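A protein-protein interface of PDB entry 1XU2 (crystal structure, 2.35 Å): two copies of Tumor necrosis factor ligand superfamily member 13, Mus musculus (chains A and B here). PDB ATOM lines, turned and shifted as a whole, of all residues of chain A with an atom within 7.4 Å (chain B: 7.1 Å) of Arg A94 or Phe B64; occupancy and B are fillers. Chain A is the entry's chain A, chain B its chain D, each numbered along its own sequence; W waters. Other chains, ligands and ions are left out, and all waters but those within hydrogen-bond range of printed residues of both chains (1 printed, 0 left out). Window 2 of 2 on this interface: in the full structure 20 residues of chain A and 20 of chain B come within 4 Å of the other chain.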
ATOM      1  N   HIS A  60       6.230   0.891 -15.855  1.00  0.00           N
ATOM      2  CA  HIS A  60       5.325   1.832 -15.207  1.00  0.00           C
ATOM      3  C   HIS A  60       3.972   1.119 -15.137  1.00  0.00           C
ATOM      4  O   HIS A  60       3.094   1.333 -15.967  1.00  0.00           O
ATOM      5  CB  HIS A  60       5.264   3.166 -15.979  1.00  0.00           C
ATOM      6  CG  HIS A  60       4.263   4.148 -15.442  1.00  0.00           C
ATOM      7  ND1 HIS A  60       3.869   4.174 -14.119  1.00  0.00           N
ATOM      8  CD2 HIS A  60       3.585   5.148 -16.053  1.00  0.00           C
ATOM      9  CE1 HIS A  60       2.983   5.139 -13.943  1.00  0.00           C
ATOM     10  NE2 HIS A  60       2.796   5.746 -15.100  1.00  0.00           N
ATOM     11  N   ASP A  61       3.842   0.256 -14.130  1.00  0.00           N
ATOM     12  CA  ASP A  61       2.862  -0.836 -14.111  1.00  0.00           C
ATOM     13  C   ASP A  61       2.671  -1.320 -12.658  1.00  0.00           C
ATOM     14  O   ASP A  61       3.655  -1.624 -11.973  1.00  0.00           O
ATOM     15  CB  ASP A  61       3.402  -1.978 -14.998  1.00  0.00           C
ATOM     16  CG  ASP A  61       2.333  -2.977 -15.424  1.00  0.00           C
ATOM     17  OD1 ASP A  61       1.566  -3.461 -14.559  1.00  0.00           O
ATOM     18  OD2 ASP A  61       2.209  -3.361 -16.608  1.00  0.00           O
ATOM     19  N   VAL A  62       1.421  -1.397 -12.189  1.00  0.00           N
ATOM     20  CA  VAL A  62       1.144  -1.749 -10.780  1.00  0.00           C
ATOM     21  C   VAL A  62       1.073  -3.255 -10.482  1.00  0.00           C
ATOM     22  O   VAL A  62       0.837  -3.649  -9.341  1.00  0.00           O
ATOM     23  CB  VAL A  62      -0.147  -1.072 -10.232  1.00  0.00           C
ATOM     24  CG1 VAL A  62      -0.037   0.438 -10.341  1.00  0.00           C
ATOM     25  CG2 VAL A  62      -1.420  -1.594 -10.932  1.00  0.00           C
ATOM     26  N   MET A  88       6.509  -4.141  -7.462  1.00  0.00           N
ATOM     27  CA  MET A  88       6.038  -2.833  -7.874  1.00  0.00           C
ATOM     28  C   MET A  88       5.087  -2.276  -6.822  1.00  0.00           C
ATOM     29  O   MET A  88       4.360  -3.024  -6.189  1.00  0.00           O
ATOM     30  CB  MET A  88       5.324  -2.911  -9.229  1.00  0.00           C
ATOM     31  CG  MET A  88       6.126  -3.547 -10.361  1.00  0.00           C
ATOM     32  SD  MET A  88       7.588  -2.634 -10.890  1.00  0.00           S
ATOM     33  CE  MET A  88       6.845  -1.090 -11.514  1.00  0.00           C
ATOM     34  N   PRO A  89       5.102  -0.961  -6.630  1.00  0.00           N
ATOM     35  CA  PRO A  89       4.075  -0.296  -5.809  1.00  0.00           C
ATOM     36  C   PRO A  89       2.698  -0.487  -6.444  1.00  0.00           C
ATOM     37  O   PRO A  89       2.598  -0.636  -7.660  1.00  0.00           O
ATOM     38  CB  PRO A  89       4.482   1.185  -5.831  1.00  0.00           C
ATOM     39  CG  PRO A  89       5.913   1.218  -6.373  1.00  0.00           C
ATOM     40  CD  PRO A  89       6.085  -0.014  -7.200  1.00  0.00           C
ATOM     41  N   SER A  90       1.657  -0.506  -5.626  1.00  0.00           N
ATOM     42  CA  SER A  90       0.297  -0.776  -6.111  1.00  0.00           C
ATOM     43  C   SER A  90      -0.455   0.500  -6.516  1.00  0.00           C
ATOM     44  O   SER A  90      -1.554   0.430  -7.069  1.00  0.00           O
ATOM     45  CB  SER A  90      -0.497  -1.540  -5.050  1.00  0.00           C
ATOM     46  OG  SER A  90      -0.274  -0.979  -3.767  1.00  0.00           O
ATOM     47  N   ASP A  91       0.152   1.655  -6.251  1.00  0.00           N
ATOM     48  CA  ASP A  91      -0.396   2.951  -6.628  1.00  0.00           C
ATOM     49  C   ASP A  91       0.129   3.314  -8.031  1.00  0.00           C
ATOM     50  O   ASP A  91       1.343   3.402  -8.218  1.00  0.00           O
ATOM     51  CB  ASP A  91       0.048   3.984  -5.591  1.00  0.00           C
ATOM     52  CG  ASP A  91      -0.837   5.198  -5.555  1.00  0.00           C
ATOM     53  OD1 ASP A  91      -0.632   6.090  -6.407  1.00  0.00           O
ATOM     54  OD2 ASP A  91      -1.747   5.350  -4.703  1.00  0.00           O
ATOM     55  N   PRO A  92      -0.758   3.514  -9.011  1.00  0.00           N
ATOM     56  CA  PRO A  92      -0.336   3.776 -10.397  1.00  0.00           C
ATOM     57  C   PRO A  92       0.653   4.931 -10.557  1.00  0.00           C
ATOM     58  O   PRO A  92       1.600   4.811 -11.309  1.00  0.00           O
ATOM     59  CB  PRO A  92      -1.656   4.116 -11.114  1.00  0.00           C
ATOM     60  CG  PRO A  92      -2.719   3.497 -10.303  1.00  0.00           C
ATOM     61  CD  PRO A  92      -2.229   3.506  -8.884  1.00  0.00           C
ATOM     62  N   ASP A  93       0.432   6.029  -9.847  1.00  0.00           N
ATOM     63  CA  ASP A  93       1.273   7.219  -9.976  1.00  0.00           C
ATOM     64  C   ASP A  93       2.682   7.031  -9.418  1.00  0.00           C
ATOM     65  O   ASP A  93       3.592   7.765  -9.784  1.00  0.00           O
ATOM     66  CB  ASP A  93       0.606   8.404  -9.278  1.00  0.00           C
ATOM     67  CG  ASP A  93      -0.673   8.822  -9.956  1.00  0.00           C
ATOM     68  OD1 ASP A  93      -0.577   9.448 -11.035  1.00  0.00           O
ATOM     69  OD2 ASP A  93      -1.811   8.564  -9.500  1.00  0.00           O
ATOM     70  N   ARG A  94       2.850   6.065  -8.523  1.00  0.00           N
ATOM     71  CA  ARG A  94       4.140   5.786  -7.889  1.00  0.00           C
ATOM     72  C   ARG A  94       4.903   4.602  -8.509  1.00  0.00           C
ATOM     73  O   ARG A  94       6.062   4.367  -8.150  1.00  0.00           O
ATOM     74  CB  ARG A  94       3.906   5.498  -6.405  1.00  0.00           C
ATOM     75  CG  ARG A  94       3.192   6.619  -5.657  1.00  0.00           C
ATOM     76  CD  ARG A  94       2.985   6.357  -4.165  1.00  0.00           C
ATOM     77  NE  ARG A  94       4.252   6.134  -3.464  1.00  0.00           N
ATOM     78  CZ  ARG A  94       4.543   6.569  -2.237  1.00  0.00           C
ATOM     79  NH1 ARG A  94       3.652   7.248  -1.513  1.00  0.00           N
ATOM     80  NH2 ARG A  94       5.736   6.299  -1.716  1.00  0.00           N
ATOM     81  N   ALA A  95       4.266   3.889  -9.448  1.00  0.00           N
ATOM     82  CA  ALA A  95       4.713   2.569  -9.891  1.00  0.00           C
ATOM     83  C   ALA A  95       5.738   2.597 -11.025  1.00  0.00           C
ATOM     84  O   ALA A  95       5.427   2.239 -12.161  1.00  0.00           O
ATOM     85  CB  ALA A  95       3.503   1.724 -10.298  1.00  0.00           C
ATOM     86  N   TYR A  96       6.964   2.995 -10.698  1.00  0.00           N
ATOM     87  CA  TYR A  96       8.066   3.007 -11.641  1.00  0.00           C
ATOM     88  C   TYR A  96       9.224   2.190 -11.096  1.00  0.00           C
ATOM     89  O   TYR A  96       9.594   2.341  -9.935  1.00  0.00           O
ATOM     90  CB  TYR A  96       8.568   4.432 -11.847  1.00  0.00           C
ATOM     91  CG  TYR A  96       7.594   5.415 -12.459  1.00  0.00           C
ATOM     92  CD1 TYR A  96       6.680   6.090 -11.668  1.00  0.00           C
ATOM     93  CD2 TYR A  96       7.628   5.710 -13.825  1.00  0.00           C
ATOM     94  CE1 TYR A  96       5.794   7.013 -12.214  1.00  0.00           C
ATOM     95  CE2 TYR A  96       6.750   6.635 -14.386  1.00  0.00           C
ATOM     96  CZ  TYR A  96       5.834   7.283 -13.568  1.00  0.00           C
ATOM     97  OH  TYR A  96       4.953   8.203 -14.082  1.00  0.00           O
ATOM     98  N   ASN A  97       9.800   1.335 -11.940  1.00  0.00           N
ATOM     99  CA  ASN A  97      11.029   0.615 -11.622  1.00  0.00           C
ATOM    100  C   ASN A  97      11.726   0.147 -12.905  1.00  0.00           C
ATOM    101  O   ASN A  97      11.080  -0.354 -13.831  1.00  0.00           O
ATOM    102  CB  ASN A  97      10.728  -0.626 -10.774  1.00  0.00           C
ATOM    103  CG  ASN A  97      10.666  -0.342  -9.287  1.00  0.00           C
ATOM    104  OD1 ASN A  97      11.575   0.243  -8.725  1.00  0.00           O
ATOM    105  ND2 ASN A  97       9.597  -0.772  -8.648  1.00  0.00           N
ATOM    106  N   ASP B  61      16.454   7.052   1.167  1.00  0.00           N
ATOM    107  CA  ASP B  61      15.627   8.201   0.815  1.00  0.00           C
ATOM    108  C   ASP B  61      14.171   7.764   0.607  1.00  0.00           C
ATOM    109  O   ASP B  61      13.914   6.789  -0.106  1.00  0.00           O
ATOM    110  CB  ASP B  61      16.178   8.783  -0.492  1.00  0.00           C
ATOM    111  CG  ASP B  61      15.926  10.262  -0.630  1.00  0.00           C
ATOM    112  OD1 ASP B  61      14.747  10.668  -0.701  1.00  0.00           O
ATOM    113  OD2 ASP B  61      16.854  11.093  -0.688  1.00  0.00           O
ATOM    114  N   VAL B  62      13.224   8.477   1.211  1.00  0.00           N
ATOM    115  CA  VAL B  62      11.806   8.103   1.136  1.00  0.00           C
ATOM    116  C   VAL B  62      11.080   8.690  -0.068  1.00  0.00           C
ATOM    117  O   VAL B  62       9.920   8.364  -0.313  1.00  0.00           O
ATOM    118  CB  VAL B  62      11.030   8.441   2.445  1.00  0.00           C
ATOM    119  CG1 VAL B  62      11.709   7.778   3.628  1.00  0.00           C
ATOM    120  CG2 VAL B  62      10.890   9.966   2.678  1.00  0.00           C
ATOM    121  N   THR B  63      11.763   9.539  -0.830  1.00  0.00           N
ATOM    122  CA  THR B  63      11.197  10.080  -2.065  1.00  0.00           C
ATOM    123  C   THR B  63      10.690   8.932  -2.940  1.00  0.00           C
ATOM    124  O   THR B  63      11.385   7.931  -3.126  1.00  0.00           O
ATOM    125  CB  THR B  63      12.235  10.936  -2.826  1.00  0.00           C
ATOM    126  OG1 THR B  63      12.661  12.034  -2.004  1.00  0.00           O
ATOM    127  CG2 THR B  63      11.610  11.606  -4.054  1.00  0.00           C
ATOM    128  N   PHE B  64       9.482   9.099  -3.468  1.00  0.00           N
ATOM    129  CA  PHE B  64       8.706   7.999  -4.041  1.00  0.00           C
ATOM    130  C   PHE B  64       9.491   7.208  -5.080  1.00  0.00           C
ATOM    131  O   PHE B  64       9.419   5.985  -5.091  1.00  0.00           O
ATOM    132  CB  PHE B  64       7.335   8.489  -4.568  1.00  0.00           C
ATOM    133  CG  PHE B  64       7.391   9.183  -5.904  1.00  0.00           C
ATOM    134  CD1 PHE B  64       7.870  10.487  -6.015  1.00  0.00           C
ATOM    135  CD2 PHE B  64       6.952   8.533  -7.057  1.00  0.00           C
ATOM    136  CE1 PHE B  64       7.924  11.125  -7.257  1.00  0.00           C
ATOM    137  CE2 PHE B  64       6.996   9.169  -8.292  1.00  0.00           C
ATOM    138  CZ  PHE B  64       7.483  10.464  -8.389  1.00  0.00           C
ATOM    139  N   THR B  65      10.242   7.906  -5.933  1.00  0.00           N
ATOM    140  CA  THR B  65      11.256   7.271  -6.768  1.00  0.00           C
ATOM    141  C   THR B  65      12.588   7.998  -6.646  1.00  0.00           C
ATOM    142  O   THR B  65      12.642   9.214  -6.445  1.00  0.00           O
ATOM    143  CB  THR B  65      10.842   7.247  -8.261  1.00  0.00           C
ATOM    144  OG1 THR B  65      10.356   8.537  -8.663  1.00  0.00           O
ATOM    145  CG2 THR B  65       9.668   6.302  -8.489  1.00  0.00           C
ATOM    146  N   MET B  66      13.658   7.223  -6.764  1.00  0.00           N
ATOM    147  CA  MET B  66      15.007   7.731  -6.852  1.00  0.00           C
ATOM    148  C   MET B  66      15.721   7.038  -8.024  1.00  0.00           C
ATOM    149  O   MET B  66      15.265   6.022  -8.554  1.00  0.00           O
ATOM    150  CB  MET B  66      15.766   7.473  -5.546  1.00  0.00           C
ATOM    151  CG  MET B  66      15.275   8.247  -4.312  1.00  0.00           C
ATOM    152  SD  MET B  66      15.325  10.075  -4.471  1.00  0.00           S
ATOM    153  CE  MET B  66      17.064  10.390  -4.500  1.00  0.00           C
ATOM    154  N   ARG B  86      14.137   3.430  -9.239  1.00  0.00           N
ATOM    155  CA  ARG B  86      13.739   2.542  -8.169  1.00  0.00           C
ATOM    156  C   ARG B  86      12.697   3.246  -7.291  1.00  0.00           C
ATOM    157  O   ARG B  86      12.933   4.333  -6.799  1.00  0.00           O
ATOM    158  CB  ARG B  86      14.991   2.150  -7.378  1.00  0.00           C
ATOM    159  CG  ARG B  86      14.912   0.851  -6.571  1.00  0.00           C
ATOM    160  CD  ARG B  86      14.406  -0.410  -7.288  1.00  0.00           C
ATOM    161  NE  ARG B  86      14.733  -0.466  -8.717  1.00  0.00           N
ATOM    162  CZ  ARG B  86      15.930  -0.749  -9.213  1.00  0.00           C
ATOM    163  NH1 ARG B  86      16.956  -0.998  -8.417  1.00  0.00           N
ATOM    164  NH2 ARG B  86      16.103  -0.773 -10.523  1.00  0.00           N
ATOM    165  N   SER B  87      11.524   2.648  -7.145  1.00  0.00           N
ATOM    166  CA  SER B  87      10.575   3.075  -6.130  1.00  0.00           C
ATOM    167  C   SER B  87      11.128   2.816  -4.723  1.00  0.00           C
ATOM    168  O   SER B  87      11.790   1.804  -4.489  1.00  0.00           O
ATOM    169  CB  SER B  87       9.264   2.335  -6.314  1.00  0.00           C
ATOM    170  OG  SER B  87       8.712   2.679  -7.576  1.00  0.00           O
ATOM    171  N   MET B  88      10.864   3.735  -3.800  1.00  0.00           N
ATOM    172  CA  MET B  88      11.380   3.629  -2.438  1.00  0.00           C
ATOM    173  C   MET B  88      10.231   3.452  -1.453  1.00  0.00           C
ATOM    174  O   MET B  88       9.155   3.969  -1.683  1.00  0.00           O
ATOM    175  CB  MET B  88      12.179   4.879  -2.070  1.00  0.00           C
ATOM    176  CG  MET B  88      13.292   5.243  -3.055  1.00  0.00           C
ATOM    177  SD  MET B  88      14.665   4.062  -3.141  1.00  0.00           S
ATOM    178  CE  MET B  88      15.266   4.038  -1.418  1.00  0.00           C
ATOM    179  N   PRO B  89      10.445   2.686  -0.381  1.00  0.00           N
ATOM    180  CA  PRO B  89       9.519   2.671   0.760  1.00  0.00           C
ATOM    181  C   PRO B  89       9.316   4.065   1.367  1.00  0.00           C
ATOM    182  O   PRO B  89      10.190   4.933   1.290  1.00  0.00           O
ATOM    183  CB  PRO B  89      10.216   1.751   1.777  1.00  0.00           C
ATOM    184  CG  PRO B  89      11.136   0.907   0.979  1.00  0.00           C
ATOM    185  CD  PRO B  89      11.556   1.736  -0.203  1.00  0.00           C
ATOM    186  N   SER B  90       8.161   4.280   1.963  1.00  0.00           N
ATOM    187  CA  SER B  90       7.836   5.592   2.522  1.00  0.00           C
ATOM    188  C   SER B  90       8.310   5.770   3.979  1.00  0.00           C
ATOM    189  O   SER B  90       8.324   6.888   4.485  1.00  0.00           O
ATOM    190  CB  SER B  90       6.341   5.842   2.396  1.00  0.00           C
ATOM    191  OG  SER B  90       5.613   4.879   3.134  1.00  0.00           O
ATOM    192  N   ARG B 119      17.098  14.794  -7.990  1.00  0.00           N
ATOM    193  CA  ARG B 119      16.475  15.396  -6.808  1.00  0.00           C
ATOM    194  C   ARG B 119      17.519  16.204  -6.057  1.00  0.00           C
ATOM    195  O   ARG B 119      18.703  15.865  -6.058  1.00  0.00           O
ATOM    196  CB  ARG B 119      15.917  14.327  -5.855  1.00  0.00           C
ATOM    197  CG  ARG B 119      14.720  13.579  -6.395  1.00  0.00           C
ATOM    198  CD  ARG B 119      15.086  12.363  -7.254  1.00  0.00           C
ATOM    199  NE  ARG B 119      13.904  11.600  -7.645  1.00  0.00           N
ATOM    200  CZ  ARG B 119      13.051  11.959  -8.594  1.00  0.00           C
ATOM    201  NH1 ARG B 119      13.258  13.058  -9.305  1.00  0.00           N
ATOM    202  NH2 ARG B 119      11.988  11.198  -8.847  1.00  0.00           N
HETATM  203  O   HOH W   1       7.194   5.108  -5.848  1.00  0.00           O
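O of Arg A94 lies within hydrogen-bond range of OG of Ser B87 (3.2 Å). O of Tyr A96 is in hydrogen-bond range of OG of Ser B87. NE of Arg B86 sits close to OD1 of Asn A97 (3.2 Å). OD1 of Asn A97 is in hydrogen-bond range of N of Ser B87.
NE2 of His A60 sits at hydrogen-bond distance from OH of Tyr A96, 3.4 Å away. The side-chain sulfur (SD) of Met A88 is in hydrogen-bond range of the side-chain amide nitrogen (ND2) of Asn A97 (3.5 Å). O of Phe B64 sits at hydrogen-bond distance from N of Met B88 (3.0 Å). NE of Arg B119 sits at hydrogen-bond distance from O of Thr B65, 3.0 Å away. The backbone carbonyl oxygen of Met B66 lies within hydrogen-bond range of the backbone NH of Arg B86, at 2.9 Å.
Among the printed residues, pairs that only touch across the chains: Pro A89 with Ser B87 (3.4 Å), Asp A93 with Phe B64 (3.97 Å), Arg A94 with Phe B64 (3.9 Å) and Tyr A96 with Thr B65 (3.998 Å).
Of the printed residues of chain B, Pro A89 touches Ser B87 (3.4 Å). Printed residues of chain B within 4 Å of Asp A93: Phe B64. Of chain B, only Phe B64 (3.9 Å) and Ser B87 (3.2 Å) come within 4 Å of Arg A94. Printed residues of chain B within 4 Å of Asn A97: Arg B86 (3.2 Å) and Ser B87 (2.9 Å). Phe B64 touches just these residues of chain A: Asp A93 and Arg A94. Printed residues of chain A within 4 Å of Arg B86: Asn A97 (3.2 Å). Printed residues of chain A within 4 Å of Ser B87: Pro A89 (3.4 Å), Arg A94 (3.2 Å), Tyr A96 (2.5 Å) and Asn A97 (2.9 Å). Met B88 touches none of the printed residues of chain A. The nearest residue of chain B that does not touch Arg A94 is Thr B65 (4.1 Å). The nearest printed residue of chain A that does not touch Arg B86 is Tyr A96 (4.2 Å).
Hydrophobic or aromatic side chains of chain B within 4 Å of the printed part of chain A: Phe B64. Along chain B the printed residues that touch a printed residue of chain A span positions 64 to 87. Among the printed residues, 8 pairs touch across the chains. Among the printed residues, no Asp or Glu carboxylate lies within 4 Å of a Lys or Arg side-chain nitrogen of the other chain.
Positions printed for both chains: 61, 62, 88, 89 and 90.
Water W1 lies within hydrogen-bond range of O of Phe B64 (2.5 Å), O of Arg A94 (2.7 Å) and OG of Ser B87 (3.3 Å).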
